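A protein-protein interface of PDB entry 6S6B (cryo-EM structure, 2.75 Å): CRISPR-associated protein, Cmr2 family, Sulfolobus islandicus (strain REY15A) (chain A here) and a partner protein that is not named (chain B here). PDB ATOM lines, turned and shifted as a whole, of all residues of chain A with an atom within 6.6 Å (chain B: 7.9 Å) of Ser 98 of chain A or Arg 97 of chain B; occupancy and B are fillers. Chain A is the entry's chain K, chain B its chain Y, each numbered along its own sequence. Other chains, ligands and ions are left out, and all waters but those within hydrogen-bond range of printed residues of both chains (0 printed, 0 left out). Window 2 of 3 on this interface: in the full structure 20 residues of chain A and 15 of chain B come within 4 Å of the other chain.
NH1 of Arg 97 of chain B is in hydrogen-bond range of OG of Ser 98 of chain A (2.7 Å).
The backbone carbonyl oxygen (O) of Gly 114 of chain A sits at hydrogen-bond distance from the side-chain amino group (NZ) of Lys 98 of chain B (2.9 Å).
The side-chain amide oxygen (OD1) of Asn 115 of chain A lies close to the backbone carbonyl oxygen (O) of Leu 95 of chain B (2.8 Å).
The guanidinium group (NH2) of Arg 32 of chain A lies close to the backbone carbonyl oxygen (O) of Arg 97 of chain A (3.3 Å).
NE of Arg 97 of chain B lies close to NE2 of His 39 of chain B, at 3.1 Å.
The backbone NH (N) of Asn 40 of chain B lies close to the backbone carbonyl oxygen (O) of Ile 96 of chain B (3.4 Å).
The backbone NH (N) of Asn 40 of chain B lies within hydrogen-bond range of the backbone carbonyl oxygen (O) of Arg 97 of chain B (2.8 Å).
The backbone NH (N) of Val 41 of chain B is in hydrogen-bond range of the backbone carbonyl oxygen (O) of Ile 96 of chain B, 2.6 Å away.
Arg 32 of chain A touches Lys 98 of chain B (CD to NZ, 3.8 Å).
Phe 100 of chain A touches Arg 97 of chain B (CE2 to NH1, 3.98 Å).
Asp 112 of chain A touches Ile 96 of chain B.
Leu 166 of chain B touches Asp 112 of chain A.
CA of Gly 114 of chain A touches O of Leu 95 of chain B, at 3.96 Å.
N of Gly 114 of chain A touches CD1 of Ile 96 of chain B, 3.4 Å away.
ND2 of Asn 115 of chain A touches CD of Lys 98 of chain B, at 3.4 Å.
Printed residues of chain B within 4 Å of Arg 32 of chain A: Lys 98 (3.8 Å).
Of chain B, only Arg 97 (2.7 Å) comes within 4 Å of Ser 98 of chain A.
Of the printed residues of chain B, Asp 112 of chain A touches Ile 96 (3.1 Å) and Leu 166 (3.2 Å).
Asn 32 of chain B touches none of the printed residues of chain A.
Printed residues of chain A within 4 Å of Ile 96 of chain B: Asp 112 (3.1 Å) and Gly 114 (3.4 Å).
Of the printed residues of chain A, Arg 97 of chain B touches Ser 98 (2.7 Å) and Phe 100 (3.98 Å).
Lys 158 of chain B touches none of the printed residues of chain A.
Of the printed residues of chain A, Leu 166 of chain B touches Asp 112 (3.2 Å).
The nearest residue of chain B that does not touch Ser 98 of chain A is Arg 36 of chain B (4.7 Å).
The nearest printed residue of chain A that does not touch Arg 97 of chain B is Gly 114 of chain A (4.9 Å).
Of the 20 printed residues of chain B, 5 touch a printed residue of chain A.
Hydrophobic or aromatic side chains of chain B within 4 Å of the printed part of chain A: Ile 96 and Leu 166.
Along chain B the printed residues that touch a printed residue of chain A span positions 95 to 166.
Printed residues of chain A that touch a printed residue of chain B: Arg 32, Ser 98, Phe 100, Asp 112, Gly 114 and Asn 115.
Hydrophobic or aromatic side chains of chain A within 4 Å of the printed part of chain B: Phe 100.
Among the printed residues, 10 pairs touch across the chains.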
ATOM      1  N   THR A  30      -0.813   3.550 -25.408  1.00  0.00           N
ATOM      2  CA  THR A  30      -2.078   2.886 -25.712  1.00  0.00           C
ATOM      3  C   THR A  30      -2.862   2.672 -24.413  1.00  0.00           C
ATOM      4  O   THR A  30      -3.153   1.553 -23.990  1.00  0.00           O
ATOM      5  CB  THR A  30      -1.835   1.578 -26.466  1.00  0.00           C
ATOM      6  OG1 THR A  30      -0.835   1.795 -27.469  1.00  0.00           O
ATOM      7  CG2 THR A  30      -3.096   1.126 -27.162  1.00  0.00           C
ATOM      8  N   ARG A  32      -4.355   2.520 -20.580  1.00  0.00           N
ATOM      9  CA  ARG A  32      -5.324   1.774 -19.786  1.00  0.00           C
ATOM     10  C   ARG A  32      -6.038   2.661 -18.776  1.00  0.00           C
ATOM     11  O   ARG A  32      -7.270   2.733 -18.772  1.00  0.00           O
ATOM     12  CB  ARG A  32      -4.634   0.620 -19.050  1.00  0.00           C
ATOM     13  CG  ARG A  32      -4.020  -0.422 -19.952  1.00  0.00           C
ATOM     14  CD  ARG A  32      -5.037  -0.958 -20.938  1.00  0.00           C
ATOM     15  NE  ARG A  32      -4.466  -2.000 -21.782  1.00  0.00           N
ATOM     16  CZ  ARG A  32      -3.606  -1.776 -22.770  1.00  0.00           C
ATOM     17  NH1 ARG A  32      -3.215  -0.541 -23.051  1.00  0.00           N
ATOM     18  NH2 ARG A  32      -3.138  -2.789 -23.480  1.00  0.00           N
ATOM     19  N   ASN A  96      -1.609  -2.445 -30.474  1.00  0.00           N
ATOM     20  CA  ASN A  96      -2.200  -3.665 -29.933  1.00  0.00           C
ATOM     21  C   ASN A  96      -2.486  -3.412 -28.466  1.00  0.00           C
ATOM     22  O   ASN A  96      -1.559  -3.180 -27.683  1.00  0.00           O
ATOM     23  CB  ASN A  96      -1.283  -4.872 -30.122  1.00  0.00           C
ATOM     24  CG  ASN A  96       0.123  -4.614 -29.652  1.00  0.00           C
ATOM     25  OD1 ASN A  96       0.610  -3.486 -29.711  1.00  0.00           O
ATOM     26  ND2 ASN A  96       0.794  -5.661 -29.188  1.00  0.00           N
ATOM     27  N   ARG A  97      -3.763  -3.432 -28.098  1.00  0.00           N
ATOM     28  CA  ARG A  97      -4.180  -3.100 -26.738  1.00  0.00           C
ATOM     29  C   ARG A  97      -4.194  -4.353 -25.862  1.00  0.00           C
ATOM     30  O   ARG A  97      -5.186  -4.695 -25.221  1.00  0.00           O
ATOM     31  CB  ARG A  97      -5.544  -2.420 -26.758  1.00  0.00           C
ATOM     32  CG  ARG A  97      -5.701  -1.366 -27.843  1.00  0.00           C
ATOM     33  CD  ARG A  97      -6.573  -0.211 -27.372  1.00  0.00           C
ATOM     34  NE  ARG A  97      -6.010   0.452 -26.200  1.00  0.00           N
ATOM     35  CZ  ARG A  97      -6.450   0.292 -24.956  1.00  0.00           C
ATOM     36  NH1 ARG A  97      -7.478  -0.509 -24.711  1.00  0.00           N
ATOM     37  NH2 ARG A  97      -5.863   0.937 -23.959  1.00  0.00           N
ATOM     38  N   SER A  98      -3.053  -5.038 -25.844  1.00  0.00           N
ATOM     39  CA  SER A  98      -2.879  -6.205 -24.982  1.00  0.00           C
ATOM     40  C   SER A  98      -1.405  -6.310 -24.625  1.00  0.00           C
ATOM     41  O   SER A  98      -0.568  -6.565 -25.496  1.00  0.00           O
ATOM     42  CB  SER A  98      -3.377  -7.475 -25.661  1.00  0.00           C
ATOM     43  OG  SER A  98      -4.780  -7.424 -25.855  1.00  0.00           O
ATOM     44  N   ILE A  99      -1.098  -6.124 -23.345  1.00  0.00           N
ATOM     45  CA  ILE A  99       0.275  -6.120 -22.862  1.00  0.00           C
ATOM     46  C   ILE A  99       0.722  -7.533 -22.523  1.00  0.00           C
ATOM     47  O   ILE A  99       0.610  -7.975 -21.375  1.00  0.00           O
ATOM     48  CB  ILE A  99       0.419  -5.200 -21.639  1.00  0.00           C
ATOM     49  CG1 ILE A  99      -0.217  -3.845 -21.927  1.00  0.00           C
ATOM     50  CG2 ILE A  99       1.878  -5.040 -21.259  1.00  0.00           C
ATOM     51  CD1 ILE A  99      -0.281  -2.948 -20.728  1.00  0.00           C
ATOM     52  N   PHE A 100       1.222  -8.253 -23.517  1.00  0.00           N
ATOM     53  CA  PHE A 100       1.920  -9.502 -23.268  1.00  0.00           C
ATOM     54  C   PHE A 100       3.390  -9.211 -23.013  1.00  0.00           C
ATOM     55  O   PHE A 100       3.917  -8.181 -23.435  1.00  0.00           O
ATOM     56  CB  PHE A 100       1.779 -10.456 -24.451  1.00  0.00           C
ATOM     57  CG  PHE A 100       0.414 -11.043 -24.590  1.00  0.00           C
ATOM     58  CD1 PHE A 100       0.028 -12.114 -23.809  1.00  0.00           C
ATOM     59  CD2 PHE A 100      -0.484 -10.527 -25.502  1.00  0.00           C
ATOM     60  CE1 PHE A 100      -1.230 -12.657 -23.931  1.00  0.00           C
ATOM     61  CE2 PHE A 100      -1.742 -11.066 -25.631  1.00  0.00           C
ATOM     62  CZ  PHE A 100      -2.117 -12.133 -24.843  1.00  0.00           C
ATOM     63  N   ASP A 112       1.108 -12.510 -19.185  1.00  0.00           N
ATOM     64  CA  ASP A 112       0.118 -11.486 -19.470  1.00  0.00           C
ATOM     65  C   ASP A 112       0.060 -10.520 -18.295  1.00  0.00           C
ATOM     66  O   ASP A 112       0.034 -10.937 -17.134  1.00  0.00           O
ATOM     67  CB  ASP A 112      -1.241 -12.113 -19.765  1.00  0.00           C
ATOM     68  CG  ASP A 112      -2.105 -11.223 -20.619  1.00  0.00           C
ATOM     69  OD1 ASP A 112      -1.687 -10.076 -20.886  1.00  0.00           O
ATOM     70  OD2 ASP A 112      -3.171 -11.685 -21.069  1.00  0.00           O
ATOM     71  N   GLY A 114      -1.839  -7.674 -17.316  1.00  0.00           N
ATOM     72  CA  GLY A 114      -3.024  -6.834 -17.383  1.00  0.00           C
ATOM     73  C   GLY A 114      -3.019  -5.497 -16.664  1.00  0.00           C
ATOM     74  O   GLY A 114      -3.006  -4.462 -17.337  1.00  0.00           O
ATOM     75  N   ASN A 115      -3.025  -5.470 -15.326  1.00  0.00           N
ATOM     76  CA  ASN A 115      -2.988  -4.182 -14.629  1.00  0.00           C
ATOM     77  C   ASN A 115      -2.493  -4.370 -13.195  1.00  0.00           C
ATOM     78  O   ASN A 115      -3.274  -4.752 -12.323  1.00  0.00           O
ATOM     79  CB  ASN A 115      -4.355  -3.517 -14.649  1.00  0.00           C
ATOM     80  CG  ASN A 115      -5.478  -4.480 -14.338  1.00  0.00           C
ATOM     81  OD1 ASN A 115      -5.248  -5.664 -14.109  1.00  0.00           O
ATOM     82  ND2 ASN A 115      -6.704  -3.975 -14.323  1.00  0.00           N
ATOM     83  N   THR A 170       4.881  -2.847 -26.578  1.00  0.00           N
ATOM     84  CA  THR A 170       3.775  -3.783 -26.713  1.00  0.00           C
ATOM     85  C   THR A 170       3.788  -4.492 -28.058  1.00  0.00           C
ATOM     86  O   THR A 170       3.246  -5.596 -28.168  1.00  0.00           O
ATOM     87  CB  THR A 170       2.451  -3.051 -26.511  1.00  0.00           C
ATOM     88  OG1 THR A 170       2.543  -2.226 -25.346  1.00  0.00           O
ATOM     89  CG2 THR A 170       1.322  -4.042 -26.314  1.00  0.00           C
ATOM     90  N   ILE B  30     -19.410 -11.907 -18.978  1.00  0.00           N
ATOM     91  CA  ILE B  30     -18.011 -11.514 -19.099  1.00  0.00           C
ATOM     92  C   ILE B  30     -17.248 -12.389 -20.090  1.00  0.00           C
ATOM     93  O   ILE B  30     -16.088 -12.084 -20.406  1.00  0.00           O
ATOM     94  CB  ILE B  30     -17.321 -11.505 -17.714  1.00  0.00           C
ATOM     95  CG1 ILE B  30     -18.090 -10.569 -16.785  1.00  0.00           C
ATOM     96  CG2 ILE B  30     -15.904 -10.974 -17.765  1.00  0.00           C
ATOM     97  CD1 ILE B  30     -17.633 -10.590 -15.357  1.00  0.00           C
ATOM     98  N   ASN B  32     -16.276 -12.502 -23.058  1.00  0.00           N
ATOM     99  CA  ASN B  32     -16.171 -11.554 -24.168  1.00  0.00           C
ATOM    100  C   ASN B  32     -15.334 -12.148 -25.303  1.00  0.00           C
ATOM    101  O   ASN B  32     -14.347 -11.576 -25.767  1.00  0.00           O
ATOM    102  CB  ASN B  32     -15.586 -10.233 -23.682  1.00  0.00           C
ATOM    103  CG  ASN B  32     -16.487  -9.522 -22.693  1.00  0.00           C
ATOM    104  OD1 ASN B  32     -16.224  -9.510 -21.491  1.00  0.00           O
ATOM    105  ND2 ASN B  32     -17.561  -8.926 -23.196  1.00  0.00           N
ATOM    106  N   GLU B  35     -14.456 -10.956 -29.883  1.00  0.00           N
ATOM    107  CA  GLU B  35     -13.409 -10.377 -30.728  1.00  0.00           C
ATOM    108  C   GLU B  35     -12.336 -11.397 -31.103  1.00  0.00           C
ATOM    109  O   GLU B  35     -12.198 -11.765 -32.274  1.00  0.00           O
ATOM    110  CB  GLU B  35     -12.779  -9.171 -30.024  1.00  0.00           C
ATOM    111  CG  GLU B  35     -13.754  -8.326 -29.226  1.00  0.00           C
ATOM    112  CD  GLU B  35     -13.082  -7.147 -28.548  1.00  0.00           C
ATOM    113  OE1 GLU B  35     -12.882  -6.109 -29.215  1.00  0.00           O
ATOM    114  OE2 GLU B  35     -12.750  -7.258 -27.350  1.00  0.00           O
ATOM    115  N   ARG B  36     -11.567 -11.870 -30.115  1.00  0.00           N
ATOM    116  CA  ARG B  36     -10.387 -12.681 -30.395  1.00  0.00           C
ATOM    117  C   ARG B  36     -10.220 -13.824 -29.399  1.00  0.00           C
ATOM    118  O   ARG B  36      -9.093 -14.263 -29.142  1.00  0.00           O
ATOM    119  CB  ARG B  36      -9.111 -11.830 -30.387  1.00  0.00           C
ATOM    120  CG  ARG B  36      -8.841 -11.016 -31.647  1.00  0.00           C
ATOM    121  CD  ARG B  36      -9.583  -9.689 -31.637  1.00  0.00           C
ATOM    122  NE  ARG B  36      -9.327  -8.920 -30.421  1.00  0.00           N
ATOM    123  CZ  ARG B  36      -8.278  -8.125 -30.238  1.00  0.00           C
ATOM    124  NH1 ARG B  36      -7.366  -7.986 -31.192  1.00  0.00           N
ATOM    125  NH2 ARG B  36      -8.140  -7.468 -29.096  1.00  0.00           N
ATOM    126  N   GLY B  37     -11.308 -14.315 -28.825  1.00  0.00           N
ATOM    127  CA  GLY B  37     -11.219 -15.359 -27.829  1.00  0.00           C
ATOM    128  C   GLY B  37     -11.491 -14.854 -26.426  1.00  0.00           C
ATOM    129  O   GLY B  37     -12.056 -13.780 -26.212  1.00  0.00           O
ATOM    130  N   ILE B  38     -11.058 -15.652 -25.450  1.00  0.00           N
ATOM    131  CA  ILE B  38     -11.395 -15.386 -24.056  1.00  0.00           C
ATOM    132  C   ILE B  38     -10.841 -14.031 -23.639  1.00  0.00           C
ATOM    133  O   ILE B  38      -9.631 -13.783 -23.709  1.00  0.00           O
ATOM    134  CB  ILE B  38     -10.879 -16.508 -23.152  1.00  0.00           C
ATOM    135  CG1 ILE B  38     -11.567 -17.828 -23.511  1.00  0.00           C
ATOM    136  CG2 ILE B  38     -11.118 -16.168 -21.690  1.00  0.00           C
ATOM    137  CD1 ILE B  38     -10.947 -19.040 -22.856  1.00  0.00           C
ATOM    138  N   HIS B  39     -11.732 -13.146 -23.202  1.00  0.00           N
ATOM    139  CA  HIS B  39     -11.390 -11.814 -22.735  1.00  0.00           C
ATOM    140  C   HIS B  39     -11.851 -11.634 -21.293  1.00  0.00           C
ATOM    141  O   HIS B  39     -12.714 -12.363 -20.796  1.00  0.00           O
ATOM    142  CB  HIS B  39     -12.034 -10.736 -23.612  1.00  0.00           C
ATOM    143  CG  HIS B  39     -11.427 -10.617 -24.974  1.00  0.00           C
ATOM    144  ND1 HIS B  39     -11.571 -11.586 -25.942  1.00  0.00           N
ATOM    145  CD2 HIS B  39     -10.702  -9.624 -25.541  1.00  0.00           C
ATOM    146  CE1 HIS B  39     -10.943 -11.206 -27.040  1.00  0.00           C
ATOM    147  NE2 HIS B  39     -10.407 -10.019 -26.823  1.00  0.00           N
ATOM    148  N   ASN B  40     -11.263 -10.637 -20.629  1.00  0.00           N
ATOM    149  CA  ASN B  40     -11.654 -10.214 -19.282  1.00  0.00           C
ATOM    150  C   ASN B  40     -11.538 -11.376 -18.289  1.00  0.00           C
ATOM    151  O   ASN B  40     -12.516 -11.869 -17.726  1.00  0.00           O
ATOM    152  CB  ASN B  40     -13.061  -9.608 -19.297  1.00  0.00           C
ATOM    153  CG  ASN B  40     -13.164  -8.399 -20.209  1.00  0.00           C
ATOM    154  OD1 ASN B  40     -12.875  -7.275 -19.803  1.00  0.00           O
ATOM    155  ND2 ASN B  40     -13.576  -8.629 -21.450  1.00  0.00           N
ATOM    156  N   VAL B  41     -10.286 -11.805 -18.105  1.00  0.00           N
ATOM    157  CA  VAL B  41      -9.970 -12.883 -17.174  1.00  0.00           C
ATOM    158  C   VAL B  41     -10.036 -12.373 -15.733  1.00  0.00           C
ATOM    159  O   VAL B  41      -9.921 -11.173 -15.458  1.00  0.00           O
ATOM    160  CB  VAL B  41      -8.582 -13.461 -17.499  1.00  0.00           C
ATOM    161  CG1 VAL B  41      -8.366 -14.806 -16.823  1.00  0.00           C
ATOM    162  CG2 VAL B  41      -8.397 -13.576 -19.009  1.00  0.00           C
ATOM    163  N   LEU B  42     -10.223 -13.307 -14.800  1.00  0.00           N
ATOM    164  CA  LEU B  42     -10.202 -13.020 -13.375  1.00  0.00           C
ATOM    165  C   LEU B  42      -9.202 -13.937 -12.689  1.00  0.00           C
ATOM    166  O   LEU B  42      -9.217 -15.154 -12.905  1.00  0.00           O
ATOM    167  CB  LEU B  42     -11.578 -13.208 -12.741  1.00  0.00           C
ATOM    168  CG  LEU B  42     -11.538 -13.103 -11.215  1.00  0.00           C
ATOM    169  CD1 LEU B  42     -11.822 -11.682 -10.748  1.00  0.00           C
ATOM    170  CD2 LEU B  42     -12.466 -14.107 -10.564  1.00  0.00           C
ATOM    171  N   ILE B  69     -12.841 -17.544 -15.453  1.00  0.00           N
ATOM    172  CA  ILE B  69     -13.728 -16.525 -16.001  1.00  0.00           C
ATOM    173  C   ILE B  69     -14.919 -16.327 -15.078  1.00  0.00           C
ATOM    174  O   ILE B  69     -15.484 -17.288 -14.541  1.00  0.00           O
ATOM    175  CB  ILE B  69     -14.179 -16.907 -17.425  1.00  0.00           C
ATOM    176  CG1 ILE B  69     -13.014 -16.761 -18.395  1.00  0.00           C
ATOM    177  CG2 ILE B  69     -15.332 -16.027 -17.887  1.00  0.00           C
ATOM    178  CD1 ILE B  69     -12.351 -15.412 -18.330  1.00  0.00           C
ATOM    179  N   LEU B  95      -7.446  -8.295 -12.778  1.00  0.00           N
ATOM    180  CA  LEU B  95      -8.062  -8.688 -14.036  1.00  0.00           C
ATOM    181  C   LEU B  95      -7.027  -8.722 -15.153  1.00  0.00           C
ATOM    182  O   LEU B  95      -5.931  -8.166 -15.044  1.00  0.00           O
ATOM    183  CB  LEU B  95      -9.212  -7.744 -14.406  1.00  0.00           C
ATOM    184  CG  LEU B  95     -10.404  -7.758 -13.447  1.00  0.00           C
ATOM    185  CD1 LEU B  95     -11.602  -7.056 -14.061  1.00  0.00           C
ATOM    186  CD2 LEU B  95     -10.757  -9.183 -13.065  1.00  0.00           C
ATOM    187  N   ILE B  96      -7.396  -9.400 -16.239  1.00  0.00           N
ATOM    188  CA  ILE B  96      -6.550  -9.571 -17.412  1.00  0.00           C
ATOM    189  C   ILE B  96      -7.420  -9.415 -18.651  1.00  0.00           C
ATOM    190  O   ILE B  96      -8.561  -9.891 -18.675  1.00  0.00           O
ATOM    191  CB  ILE B  96      -5.850 -10.948 -17.414  1.00  0.00           C
ATOM    192  CG1 ILE B  96      -4.951 -11.104 -16.184  1.00  0.00           C
ATOM    193  CG2 ILE B  96      -5.055 -11.140 -18.680  1.00  0.00           C
ATOM    194  CD1 ILE B  96      -3.673 -10.314 -16.258  1.00  0.00           C
ATOM    195  N   ARG B  97      -6.887  -8.744 -19.676  1.00  0.00           N
ATOM    196  CA  ARG B  97      -7.602  -8.526 -20.936  1.00  0.00           C
ATOM    197  C   ARG B  97      -8.890  -7.736 -20.696  1.00  0.00           C
ATOM    198  O   ARG B  97      -9.984  -8.135 -21.100  1.00  0.00           O
ATOM    199  CB  ARG B  97      -7.885  -9.854 -21.649  1.00  0.00           C
ATOM    200  CG  ARG B  97      -8.335  -9.720 -23.100  1.00  0.00           C
ATOM    201  CD  ARG B  97      -7.171  -9.669 -24.077  1.00  0.00           C
ATOM    202  NE  ARG B  97      -7.625  -9.838 -25.456  1.00  0.00           N
ATOM    203  CZ  ARG B  97      -6.818  -9.973 -26.504  1.00  0.00           C
ATOM    204  NH1 ARG B  97      -5.503  -9.964 -26.340  1.00  0.00           N
ATOM    205  NH2 ARG B  97      -7.326 -10.121 -27.718  1.00  0.00           N
ATOM    206  N   LYS B  98      -8.749  -6.601 -20.020  1.00  0.00           N
ATOM    207  CA  LYS B  98      -9.898  -5.774 -19.682  1.00  0.00           C
ATOM    208  C   LYS B  98     -10.302  -4.902 -20.863  1.00  0.00           C
ATOM    209  O   LYS B  98      -9.456  -4.416 -21.619  1.00  0.00           O
ATOM    210  CB  LYS B  98      -9.582  -4.903 -18.469  1.00  0.00           C
ATOM    211  CG  LYS B  98      -8.394  -3.992 -18.674  1.00  0.00           C
ATOM    212  CD  LYS B  98      -7.942  -3.362 -17.375  1.00  0.00           C
ATOM    213  CE  LYS B  98      -6.699  -2.523 -17.599  1.00  0.00           C
ATOM    214  NZ  LYS B  98      -5.564  -3.366 -18.066  1.00  0.00           N
ATOM    215  N   LYS B  99     -11.607  -4.716 -21.020  1.00  0.00           N
ATOM    216  CA  LYS B  99     -12.167  -3.865 -22.053  1.00  0.00           C
ATOM    217  C   LYS B  99     -12.512  -2.511 -21.434  1.00  0.00           C
ATOM    218  O   LYS B  99     -12.079  -2.190 -20.323  1.00  0.00           O
ATOM    219  CB  LYS B  99     -13.376  -4.550 -22.694  1.00  0.00           C
ATOM    220  CG  LYS B  99     -13.662  -4.118 -24.125  1.00  0.00           C
ATOM    221  CD  LYS B  99     -14.701  -5.013 -24.772  1.00  0.00           C
ATOM    222  CE  LYS B  99     -16.025  -4.942 -24.031  1.00  0.00           C
ATOM    223  NZ  LYS B  99     -16.633  -3.588 -24.111  1.00  0.00           N
ATOM    224  N   GLY B 100     -13.263  -1.691 -22.172  1.00  0.00           N
ATOM    225  CA  GLY B 100     -13.759  -0.425 -21.667  1.00  0.00           C
ATOM    226  C   GLY B 100     -14.274  -0.529 -20.247  1.00  0.00           C
ATOM    227  O   GLY B 100     -15.008  -1.465 -19.916  1.00  0.00           O
ATOM    228  N   LYS B 158      -8.323 -20.271 -31.688  1.00  0.00           N
ATOM    229  CA  LYS B 158      -7.866 -19.200 -30.812  1.00  0.00           C
ATOM    230  C   LYS B 158      -8.381 -19.338 -29.386  1.00  0.00           C
ATOM    231  O   LYS B 158      -7.623 -19.114 -28.437  1.00  0.00           O
ATOM    232  CB  LYS B 158      -8.292 -17.840 -31.376  1.00  0.00           C
ATOM    233  CG  LYS B 158      -7.560 -16.660 -30.759  1.00  0.00           C
ATOM    234  CD  LYS B 158      -7.449 -15.500 -31.734  1.00  0.00           C
ATOM    235  CE  LYS B 158      -6.295 -14.580 -31.367  1.00  0.00           C
ATOM    236  NZ  LYS B 158      -6.530 -13.883 -30.070  1.00  0.00           N
ATOM    237  N   ASP B 162      -6.272 -20.108 -25.085  1.00  0.00           N
ATOM    238  CA  ASP B 162      -6.339 -19.282 -23.885  1.00  0.00           C
ATOM    239  C   ASP B 162      -6.555 -20.111 -22.625  1.00  0.00           C
ATOM    240  O   ASP B 162      -6.458 -19.581 -21.515  1.00  0.00           O
ATOM    241  CB  ASP B 162      -7.441 -18.231 -24.021  1.00  0.00           C
ATOM    242  CG  ASP B 162      -7.214 -17.299 -25.195  1.00  0.00           C
ATOM    243  OD1 ASP B 162      -6.301 -16.452 -25.109  1.00  0.00           O
ATOM    244  OD2 ASP B 162      -7.947 -17.408 -26.199  1.00  0.00           O
ATOM    245  N   LEU B 166      -3.618 -18.476 -20.550  1.00  0.00           N
ATOM    246  CA  LEU B 166      -4.003 -17.524 -19.518  1.00  0.00           C
ATOM    247  C   LEU B 166      -4.138 -18.170 -18.146  1.00  0.00           C
ATOM    248  O   LEU B 166      -3.471 -17.755 -17.194  1.00  0.00           O
ATOM    249  CB  LEU B 166      -5.321 -16.833 -19.909  1.00  0.00           C
ATOM    250  CG  LEU B 166      -5.316 -15.636 -20.870  1.00  0.00           C
ATOM    251  CD1 LEU B 166      -4.633 -14.440 -20.231  1.00  0.00           C
ATOM    252  CD2 LEU B 166      -4.689 -15.959 -22.220  1.00  0.00           C
